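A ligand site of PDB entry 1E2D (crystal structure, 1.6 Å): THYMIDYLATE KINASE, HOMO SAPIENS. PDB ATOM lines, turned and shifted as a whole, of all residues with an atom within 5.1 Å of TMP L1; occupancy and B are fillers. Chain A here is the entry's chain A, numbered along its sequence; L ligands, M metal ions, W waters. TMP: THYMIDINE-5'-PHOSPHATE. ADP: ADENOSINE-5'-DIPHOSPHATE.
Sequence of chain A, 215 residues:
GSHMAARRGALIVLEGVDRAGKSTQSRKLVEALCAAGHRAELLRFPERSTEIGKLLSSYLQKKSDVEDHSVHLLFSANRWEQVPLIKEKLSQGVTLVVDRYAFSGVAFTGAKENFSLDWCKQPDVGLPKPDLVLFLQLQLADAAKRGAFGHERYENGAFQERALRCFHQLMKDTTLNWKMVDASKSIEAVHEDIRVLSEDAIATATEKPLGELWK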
ATOM      1  N   LYS A  22       4.240 -15.084 -11.263  1.00  0.00           N
ATOM      2  CA  LYS A  22       4.379 -13.723 -11.769  1.00  0.00           C
ATOM      3  C   LYS A  22       3.034 -13.054 -12.032  1.00  0.00           C
ATOM      4  O   LYS A  22       2.776 -11.873 -11.741  1.00  0.00           O
ATOM      5  CB  LYS A  22       5.139 -13.783 -13.123  1.00  0.00           C
ATOM      6  CG  LYS A  22       6.605 -14.188 -12.931  1.00  0.00           C
ATOM      7  CD  LYS A  22       7.270 -14.341 -14.298  1.00  0.00           C
ATOM      8  CE  LYS A  22       6.668 -15.430 -15.179  1.00  0.00           C
ATOM      9  NZ  LYS A  22       6.896 -16.812 -14.600  1.00  0.00           N
ATOM     10  N   SER A  23       2.159 -13.790 -12.710  1.00  0.00           N
ATOM     11  CA  SER A  23       0.863 -13.157 -13.060  1.00  0.00           C
ATOM     12  C   SER A  23      -0.062 -12.984 -11.846  1.00  0.00           C
ATOM     13  O   SER A  23      -0.682 -11.921 -11.700  1.00  0.00           O
ATOM     14  CB  SER A  23       0.183 -13.945 -14.151  1.00  0.00           C
ATOM     15  OG  SER A  23       1.039 -14.006 -15.301  1.00  0.00           O
ATOM     16  N   PHE A  45       4.239  -8.362 -20.619  1.00  0.00           N
ATOM     17  CA  PHE A  45       4.892  -8.571 -21.911  1.00  0.00           C
ATOM     18  C   PHE A  45       5.015 -10.067 -22.068  1.00  0.00           C
ATOM     19  O   PHE A  45       5.351 -10.751 -21.095  1.00  0.00           O
ATOM     20  CB  PHE A  45       6.253  -7.870 -22.000  1.00  0.00           C
ATOM     21  CG  PHE A  45       6.058  -6.370 -22.011  1.00  0.00           C
ATOM     22  CD1 PHE A  45       5.638  -5.768 -23.206  1.00  0.00           C
ATOM     23  CD2 PHE A  45       6.283  -5.633 -20.878  1.00  0.00           C
ATOM     24  CE1 PHE A  45       5.448  -4.395 -23.213  1.00  0.00           C
ATOM     25  CE2 PHE A  45       6.069  -4.265 -20.919  1.00  0.00           C
ATOM     26  CZ  PHE A  45       5.646  -3.627 -22.080  1.00  0.00           C
ATOM     27  N   PRO A  46       4.726 -10.569 -23.262  1.00  0.00           N
ATOM     28  CA  PRO A  46       4.322  -9.781 -24.401  1.00  0.00           C
ATOM     29  C   PRO A  46       2.924  -9.179 -24.227  1.00  0.00           C
ATOM     30  O   PRO A  46       2.093  -9.766 -23.538  1.00  0.00           O
ATOM     31  CB  PRO A  46       4.284 -10.777 -25.565  1.00  0.00           C
ATOM     32  CG  PRO A  46       4.035 -12.096 -24.877  1.00  0.00           C
ATOM     33  CD  PRO A  46       4.810 -12.001 -23.605  1.00  0.00           C
ATOM     34  N   ARG A  48      -0.064  -8.848 -26.090  1.00  0.00           N
ATOM     35  CA  ARG A  48      -0.523  -9.521 -27.326  1.00  0.00           C
ATOM     36  C   ARG A  48      -1.583  -8.809 -28.115  1.00  0.00           C
ATOM     37  O   ARG A  48      -2.041  -9.340 -29.141  1.00  0.00           O
ATOM     38  CB  ARG A  48      -0.989 -10.918 -26.873  1.00  0.00           C
ATOM     39  CG  ARG A  48       0.002 -11.759 -26.105  1.00  0.00           C
ATOM     40  CD  ARG A  48      -0.541 -13.146 -25.834  1.00  0.00           C
ATOM     41  NE  ARG A  48       0.336 -13.913 -24.966  1.00  0.00           N
ATOM     42  CZ  ARG A  48       0.615 -15.199 -25.221  1.00  0.00           C
ATOM     43  NH1 ARG A  48       0.114 -15.845 -26.262  1.00  0.00           N
ATOM     44  NH2 ARG A  48       1.416 -15.786 -24.338  1.00  0.00           N
ATOM     45  N   LEU A  60       3.987 -18.143 -29.955  1.00  0.00           N
ATOM     46  CA  LEU A  60       4.042 -18.867 -28.680  1.00  0.00           C
ATOM     47  C   LEU A  60       3.062 -20.025 -28.574  1.00  0.00           C
ATOM     48  O   LEU A  60       3.287 -20.938 -27.783  1.00  0.00           O
ATOM     49  CB  LEU A  60       3.741 -17.851 -27.565  1.00  0.00           C
ATOM     50  CG  LEU A  60       4.888 -16.846 -27.364  1.00  0.00           C
ATOM     51  CD1 LEU A  60       4.378 -15.721 -26.450  1.00  0.00           C
ATOM     52  CD2 LEU A  60       6.111 -17.534 -26.783  1.00  0.00           C
ATOM     53  N   PHE A  75       9.748  -9.329 -29.949  1.00  0.00           N
ATOM     54  CA  PHE A  75       9.508  -9.192 -28.501  1.00  0.00           C
ATOM     55  C   PHE A  75      10.015  -7.861 -27.974  1.00  0.00           C
ATOM     56  O   PHE A  75       9.387  -7.203 -27.139  1.00  0.00           O
ATOM     57  CB  PHE A  75      10.206 -10.338 -27.734  1.00  0.00           C
ATOM     58  CG  PHE A  75       9.372 -11.574 -27.612  1.00  0.00           C
ATOM     59  CD1 PHE A  75       8.198 -11.593 -26.852  1.00  0.00           C
ATOM     60  CD2 PHE A  75       9.801 -12.758 -28.197  1.00  0.00           C
ATOM     61  CE1 PHE A  75       7.464 -12.759 -26.720  1.00  0.00           C
ATOM     62  CE2 PHE A  75       9.050 -13.911 -28.087  1.00  0.00           C
ATOM     63  CZ  PHE A  75       7.861 -13.935 -27.365  1.00  0.00           C
ATOM     64  N   ARG A  79       7.897  -4.249 -26.598  1.00  0.00           N
ATOM     65  CA  ARG A  79       8.160  -3.374 -25.445  1.00  0.00           C
ATOM     66  C   ARG A  79       8.276  -1.908 -25.881  1.00  0.00           C
ATOM     67  O   ARG A  79       7.690  -1.004 -25.262  1.00  0.00           O
ATOM     68  CB  ARG A  79       9.415  -3.781 -24.659  1.00  0.00           C
ATOM     69  CG  ARG A  79       9.107  -5.012 -23.784  1.00  0.00           C
ATOM     70  CD  ARG A  79      10.340  -5.508 -23.079  1.00  0.00           C
ATOM     71  NE  ARG A  79      11.416  -6.100 -23.924  1.00  0.00           N
ATOM     72  CZ  ARG A  79      11.342  -7.364 -24.352  1.00  0.00           C
ATOM     73  NH1 ARG A  79      10.274  -8.092 -24.074  1.00  0.00           N
ATOM     74  NH2 ARG A  79      12.399  -7.900 -25.037  1.00  0.00           N
ATOM     75  N   ASP A  99       4.369  -7.654 -15.635  1.00  0.00           N
ATOM     76  CA  ASP A  99       4.528  -9.102 -15.653  1.00  0.00           C
ATOM     77  C   ASP A  99       5.388  -9.520 -16.829  1.00  0.00           C
ATOM     78  O   ASP A  99       4.944  -9.524 -17.968  1.00  0.00           O
ATOM     79  CB  ASP A  99       3.097  -9.664 -15.721  1.00  0.00           C
ATOM     80  CG  ASP A  99       2.990 -11.160 -15.744  1.00  0.00           C
ATOM     81  OD1 ASP A  99       4.001 -11.886 -15.664  1.00  0.00           O
ATOM     82  OD2 ASP A  99       1.820 -11.625 -15.872  1.00  0.00           O
ATOM     83  N   ARG A 100       6.677  -9.691 -16.566  1.00  0.00           N
ATOM     84  CA  ARG A 100       7.756  -9.905 -17.491  1.00  0.00           C
ATOM     85  C   ARG A 100       8.158  -8.613 -18.221  1.00  0.00           C
ATOM     86  O   ARG A 100       7.377  -7.708 -18.476  1.00  0.00           O
ATOM     87  CB  ARG A 100       7.436 -10.931 -18.590  1.00  0.00           C
ATOM     88  CG  ARG A 100       7.247 -12.345 -18.052  1.00  0.00           C
ATOM     89  CD  ARG A 100       7.237 -13.308 -19.241  1.00  0.00           C
ATOM     90  NE  ARG A 100       6.806 -14.680 -18.908  1.00  0.00           N
ATOM     91  CZ  ARG A 100       7.652 -15.615 -18.493  1.00  0.00           C
ATOM     92  NH1 ARG A 100       8.958 -15.413 -18.301  1.00  0.00           N
ATOM     93  NH2 ARG A 100       7.138 -16.828 -18.273  1.00  0.00           N
ATOM     94  N   TYR A 101       9.468  -8.588 -18.529  1.00  0.00           N
ATOM     95  CA  TYR A 101      10.008  -7.401 -19.251  1.00  0.00           C
ATOM     96  C   TYR A 101      11.171  -7.849 -20.090  1.00  0.00           C
ATOM     97  O   TYR A 101      11.212  -8.968 -20.616  1.00  0.00           O
ATOM     98  CB  TYR A 101      10.375  -6.316 -18.221  1.00  0.00           C
ATOM     99  CG  TYR A 101      10.596  -4.871 -18.658  1.00  0.00           C
ATOM    100  CD1 TYR A 101       9.607  -4.226 -19.402  1.00  0.00           C
ATOM    101  CD2 TYR A 101      11.738  -4.147 -18.300  1.00  0.00           C
ATOM    102  CE1 TYR A 101       9.769  -2.896 -19.777  1.00  0.00           C
ATOM    103  CE2 TYR A 101      11.917  -2.811 -18.661  1.00  0.00           C
ATOM    104  CZ  TYR A 101      10.917  -2.214 -19.415  1.00  0.00           C
ATOM    105  OH  TYR A 101      11.018  -0.883 -19.811  1.00  0.00           O
ATOM    106  N   SER A 104      13.084 -11.374 -19.439  1.00  0.00           N
ATOM    107  CA  SER A 104      12.518 -12.580 -20.029  1.00  0.00           C
ATOM    108  C   SER A 104      12.945 -12.600 -21.513  1.00  0.00           C
ATOM    109  O   SER A 104      13.349 -13.633 -22.023  1.00  0.00           O
ATOM    110  CB  SER A 104      11.000 -12.657 -19.972  1.00  0.00           C
ATOM    111  OG  SER A 104      10.533 -13.211 -18.719  1.00  0.00           O
ATOM    112  N   GLY A 105      12.897 -11.409 -22.112  1.00  0.00           N
ATOM    113  CA  GLY A 105      13.341 -11.326 -23.531  1.00  0.00           C
ATOM    114  C   GLY A 105      14.717 -11.920 -23.710  1.00  0.00           C
ATOM    115  O   GLY A 105      15.007 -12.738 -24.611  1.00  0.00           O
ATOM    116  N   PHE A 108      15.029 -16.023 -22.592  1.00  0.00           N
ATOM    117  CA  PHE A 108      14.384 -16.988 -23.460  1.00  0.00           C
ATOM    118  C   PHE A 108      15.126 -17.101 -24.784  1.00  0.00           C
ATOM    119  O   PHE A 108      15.423 -18.225 -25.197  1.00  0.00           O
ATOM    120  CB  PHE A 108      12.881 -16.653 -23.583  1.00  0.00           C
ATOM    121  CG  PHE A 108      12.171 -17.292 -22.399  1.00  0.00           C
ATOM    122  CD1 PHE A 108      12.179 -16.670 -21.170  1.00  0.00           C
ATOM    123  CD2 PHE A 108      11.519 -18.510 -22.550  1.00  0.00           C
ATOM    124  CE1 PHE A 108      11.536 -17.253 -20.062  1.00  0.00           C
ATOM    125  CE2 PHE A 108      10.872 -19.069 -21.462  1.00  0.00           C
ATOM    126  CZ  PHE A 108      10.892 -18.454 -20.224  1.00  0.00           C
ATOM    127  N   ARG A 153       4.894 -22.808 -26.718  1.00  0.00           N
ATOM    128  CA  ARG A 153       6.336 -22.721 -26.957  1.00  0.00           C
ATOM    129  C   ARG A 153       7.104 -22.622 -25.648  1.00  0.00           C
ATOM    130  O   ARG A 153       6.651 -22.002 -24.674  1.00  0.00           O
ATOM    131  CB  ARG A 153       6.545 -21.453 -27.792  1.00  0.00           C
ATOM    132  CG  ARG A 153       7.933 -21.246 -28.339  1.00  0.00           C
ATOM    133  CD  ARG A 153       8.075 -21.763 -29.759  1.00  0.00           C
ATOM    134  NE  ARG A 153       7.124 -21.350 -30.773  1.00  0.00           N
ATOM    135  CZ  ARG A 153       7.168 -21.945 -31.989  1.00  0.00           C
ATOM    136  NH1 ARG A 153       8.101 -22.900 -32.117  1.00  0.00           N
ATOM    137  NH2 ARG A 153       6.345 -21.663 -32.956  1.00  0.00           N
ATOM    138  N   TYR A 154       8.258 -23.259 -25.538  1.00  0.00           N
ATOM    139  CA  TYR A 154       9.124 -23.192 -24.387  1.00  0.00           C
ATOM    140  C   TYR A 154       8.628 -23.971 -23.155  1.00  0.00           C
ATOM    141  O   TYR A 154       9.316 -23.926 -22.128  1.00  0.00           O
ATOM    142  CB  TYR A 154       9.424 -21.738 -23.974  1.00  0.00           C
ATOM    143  CG  TYR A 154       9.862 -20.817 -25.101  1.00  0.00           C
ATOM    144  CD1 TYR A 154      10.760 -21.287 -26.038  1.00  0.00           C
ATOM    145  CD2 TYR A 154       9.399 -19.502 -25.211  1.00  0.00           C
ATOM    146  CE1 TYR A 154      11.187 -20.486 -27.086  1.00  0.00           C
ATOM    147  CE2 TYR A 154       9.856 -18.692 -26.241  1.00  0.00           C
ATOM    148  CZ  TYR A 154      10.730 -19.203 -27.197  1.00  0.00           C
ATOM    149  OH  TYR A 154      11.173 -18.397 -28.207  1.00  0.00           O
HETATM  150  P   TMP L   1       3.868 -15.775 -19.958  1.00  0.00           P
HETATM  151  O1P TMP L   1       4.426 -17.034 -19.352  1.00  0.00           O
HETATM  152  O2P TMP L   1       4.109 -14.494 -19.259  1.00  0.00           O
HETATM  153  O3P TMP L   1       2.394 -16.049 -20.373  1.00  0.00           O
HETATM  154  O5' TMP L   1       4.625 -15.471 -21.347  1.00  0.00           O
HETATM  155  C5' TMP L   1       4.558 -16.276 -22.520  1.00  0.00           C
HETATM  156  C4' TMP L   1       5.965 -16.562 -23.054  1.00  0.00           C
HETATM  157  O4' TMP L   1       6.744 -15.510 -23.718  1.00  0.00           O
HETATM  158  C3' TMP L   1       6.872 -17.279 -22.068  1.00  0.00           C
HETATM  159  O3' TMP L   1       7.322 -18.536 -22.596  1.00  0.00           O
HETATM  160  C2' TMP L   1       8.110 -16.359 -22.021  1.00  0.00           C
HETATM  161  C1' TMP L   1       8.067 -15.696 -23.416  1.00  0.00           C
HETATM  162  N1  TMP L   1       8.856 -14.504 -23.641  1.00  0.00           N
HETATM  163  C2  TMP L   1       9.869 -14.505 -24.626  1.00  0.00           C
HETATM  164  O2  TMP L   1      10.271 -15.550 -25.165  1.00  0.00           O
HETATM  165  N3  TMP L   1      10.403 -13.255 -24.836  1.00  0.00           N
HETATM  166  C4  TMP L   1       9.961 -12.092 -24.248  1.00  0.00           C
HETATM  167  O4  TMP L   1      10.478 -10.850 -24.505  1.00  0.00           O
HETATM  168  C5  TMP L   1       8.892 -12.177 -23.236  1.00  0.00           C
HETATM  169  C5M TMP L   1       8.386 -10.928 -22.623  1.00  0.00           C
HETATM  170  C6  TMP L   1       8.335 -13.420 -23.032  1.00  0.00           C
HETATM  171  PB  ADP L   2       3.397 -17.477 -13.674  1.00  0.00           P
HETATM  172  O1B ADP L   2       4.702 -17.239 -13.006  1.00  0.00           O
HETATM  173  O2B ADP L   2       2.781 -16.329 -14.336  1.00  0.00           O
HETATM  174  O3B ADP L   2       3.508 -18.650 -14.745  1.00  0.00           O
HETATM  175  PA  ADP L   2       0.864 -17.984 -12.237  1.00  0.00           P
HETATM  176  O1A ADP L   2       0.012 -18.087 -13.450  1.00  0.00           O
HETATM  177  O2A ADP L   2       0.716 -16.712 -11.449  1.00  0.00           O
HETATM  178  O3A ADP L   2       2.419 -18.160 -12.589  1.00  0.00           O
HETATM  179  O5' ADP L   2       0.593 -19.188 -11.274  1.00  0.00           O
HETATM  180  C5' ADP L   2       0.766 -20.566 -11.748  1.00  0.00           C
HETATM  181  C4' ADP L   2      -0.231 -21.438 -10.960  1.00  0.00           C
HETATM  182  O4' ADP L   2       0.270 -21.660  -9.635  1.00  0.00           O
HETATM  183  C3' ADP L   2      -1.600 -20.815 -10.890  1.00  0.00           C
HETATM  184  O3' ADP L   2      -2.594 -21.829 -10.909  1.00  0.00           O
HETATM  185  C2' ADP L   2      -1.575 -20.198  -9.467  1.00  0.00           C
HETATM  186  O2' ADP L   2      -2.839 -20.208  -8.894  1.00  0.00           O
HETATM  187  C1' ADP L   2      -0.646 -21.150  -8.707  1.00  0.00           C
HETATM  188  N9  ADP L   2       0.117 -20.386  -7.700  1.00  0.00           N
HETATM  189  C8  ADP L   2       0.767 -19.185  -7.927  1.00  0.00           C
HETATM  190  N7  ADP L   2       1.462 -18.783  -6.878  1.00  0.00           N
HETATM  191  C5  ADP L   2       1.264 -19.809  -5.904  1.00  0.00           C
HETATM  192  C6  ADP L   2       1.712 -19.994  -4.594  1.00  0.00           C
HETATM  193  N6  ADP L   2       2.458 -19.164  -3.923  1.00  0.00           N
HETATM  194  N1  ADP L   2       1.257 -21.112  -4.019  1.00  0.00           N
HETATM  195  C2  ADP L   2       0.458 -22.023  -4.598  1.00  0.00           C
HETATM  196  N3  ADP L   2      -0.015 -21.923  -5.826  1.00  0.00           N
HETATM  197  C4  ADP L   2       0.420 -20.784  -6.378  1.00  0.00           C
HETATM  198 MG    MG M   1       2.028 -15.705 -16.120  1.00  0.00          MG
HETATM  199 MG    MG M   2       1.907 -20.052 -20.319  1.00  0.00          MG
HETATM  200  O   HOH W   1       1.353 -18.047 -21.265  1.00  0.00           O
HETATM  201  O   HOH W   2       3.607 -14.392 -16.644  1.00  0.00           O
HETATM  202  O   HOH W   3       2.630 -18.494 -24.151  1.00  0.00           O
HETATM  203  O   HOH W   4       3.004 -17.300 -17.130  1.00  0.00           O
HETATM  204  O   HOH W   5       1.083 -15.159 -17.929  1.00  0.00           O
HETATM  205  O   HOH W   6       5.387 -19.954 -23.428  1.00  0.00           O
HETATM  206  O   HOH W   7       3.250 -12.143 -19.682  1.00  0.00           O
HETATM  207  O   HOH W   8      12.752 -12.827 -26.509  1.00  0.00           O
HETATM  208  O   HOH W   9       7.792 -20.324 -20.479  1.00  0.00           O
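Residues that only touch TMP L1: Phe 45, Pro 46, Arg 48, Leu 60, Phe 75, Tyr 101, Ser 104, Phe 108 and Tyr 154. Hydrophobic or aromatic side chains within 4 Å of TMP L1: Phe 45, Pro 46, Leu 60, Phe 75, Phe 108 and Tyr 154. Within 4 Å of TMP L1: Phe 45, Pro 46, Arg 48, Leu 60, Phe 75, Arg 79, Arg 100, Tyr 101, Ser 104, Gly 105, Phe 108 and Tyr 154. The nearest printed residue that does not touch TMP L1 is Arg 153 (4.1 Å).
NZ of Lys 22 lies within salt-bridge range of O1B of ADP L2, 2.7 Å away. N of Ser 23 sits at hydrogen-bond distance from O2A of ADP L2 (3.5 Å). The backbone NH of Lys 22 sits at hydrogen-bond distance from an oxygen (O1B) of ADP L2 (2.8 Å). N of Gly 105 lies close to O4 of TMP L1 (3.4 Å). The guanidinium group (NH1) of Arg 79 lies within hydrogen-bond range of an oxygen (O4) of TMP L1 (2.8 Å). An oxygen (O2P) of TMP L1 is in salt-bridge range of the guanidinium group (NE) of Arg 100 (2.7 Å).
The backbone carbonyl oxygen (O) of Phe 75 lies within hydrogen-bond range of the guanidinium group (NH1) of Arg 79 (3.3 Å). The backbone carbonyl oxygen of Leu 60 lies within hydrogen-bond range of the backbone NH of Arg 153 (2.7 Å). The backbone NH (N) of Phe 45 sits at hydrogen-bond distance from the backbone carbonyl oxygen (O) of Asp 99 (3.0 Å). The side-chain hydroxyl (OG) of Ser 104 is in hydrogen-bond range of the guanidinium group (NH1) of Arg 100 (2.7 Å).
Water W7 lies within hydrogen-bond range of O2P of TMP L1 (2.5 Å) and O of Phe 45 (2.9 Å). Water W6 lies within hydrogen-bond range of O3' of TMP L1 and O of Arg 153. Water W4 lies within hydrogen-bond range of O1P of TMP L1 and O3B of ADP L2. Water W2 bridges an oxygen (O2P) of TMP L1 (2.7 Å) and the side-chain carboxylate (OD1) of Asp 99 (2.7 Å). Water W8 bridges a nitrogen (N3) of TMP L1 (2.9 Å) and the backbone carbonyl oxygen (O) of Gly 105 (2.9 Å).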
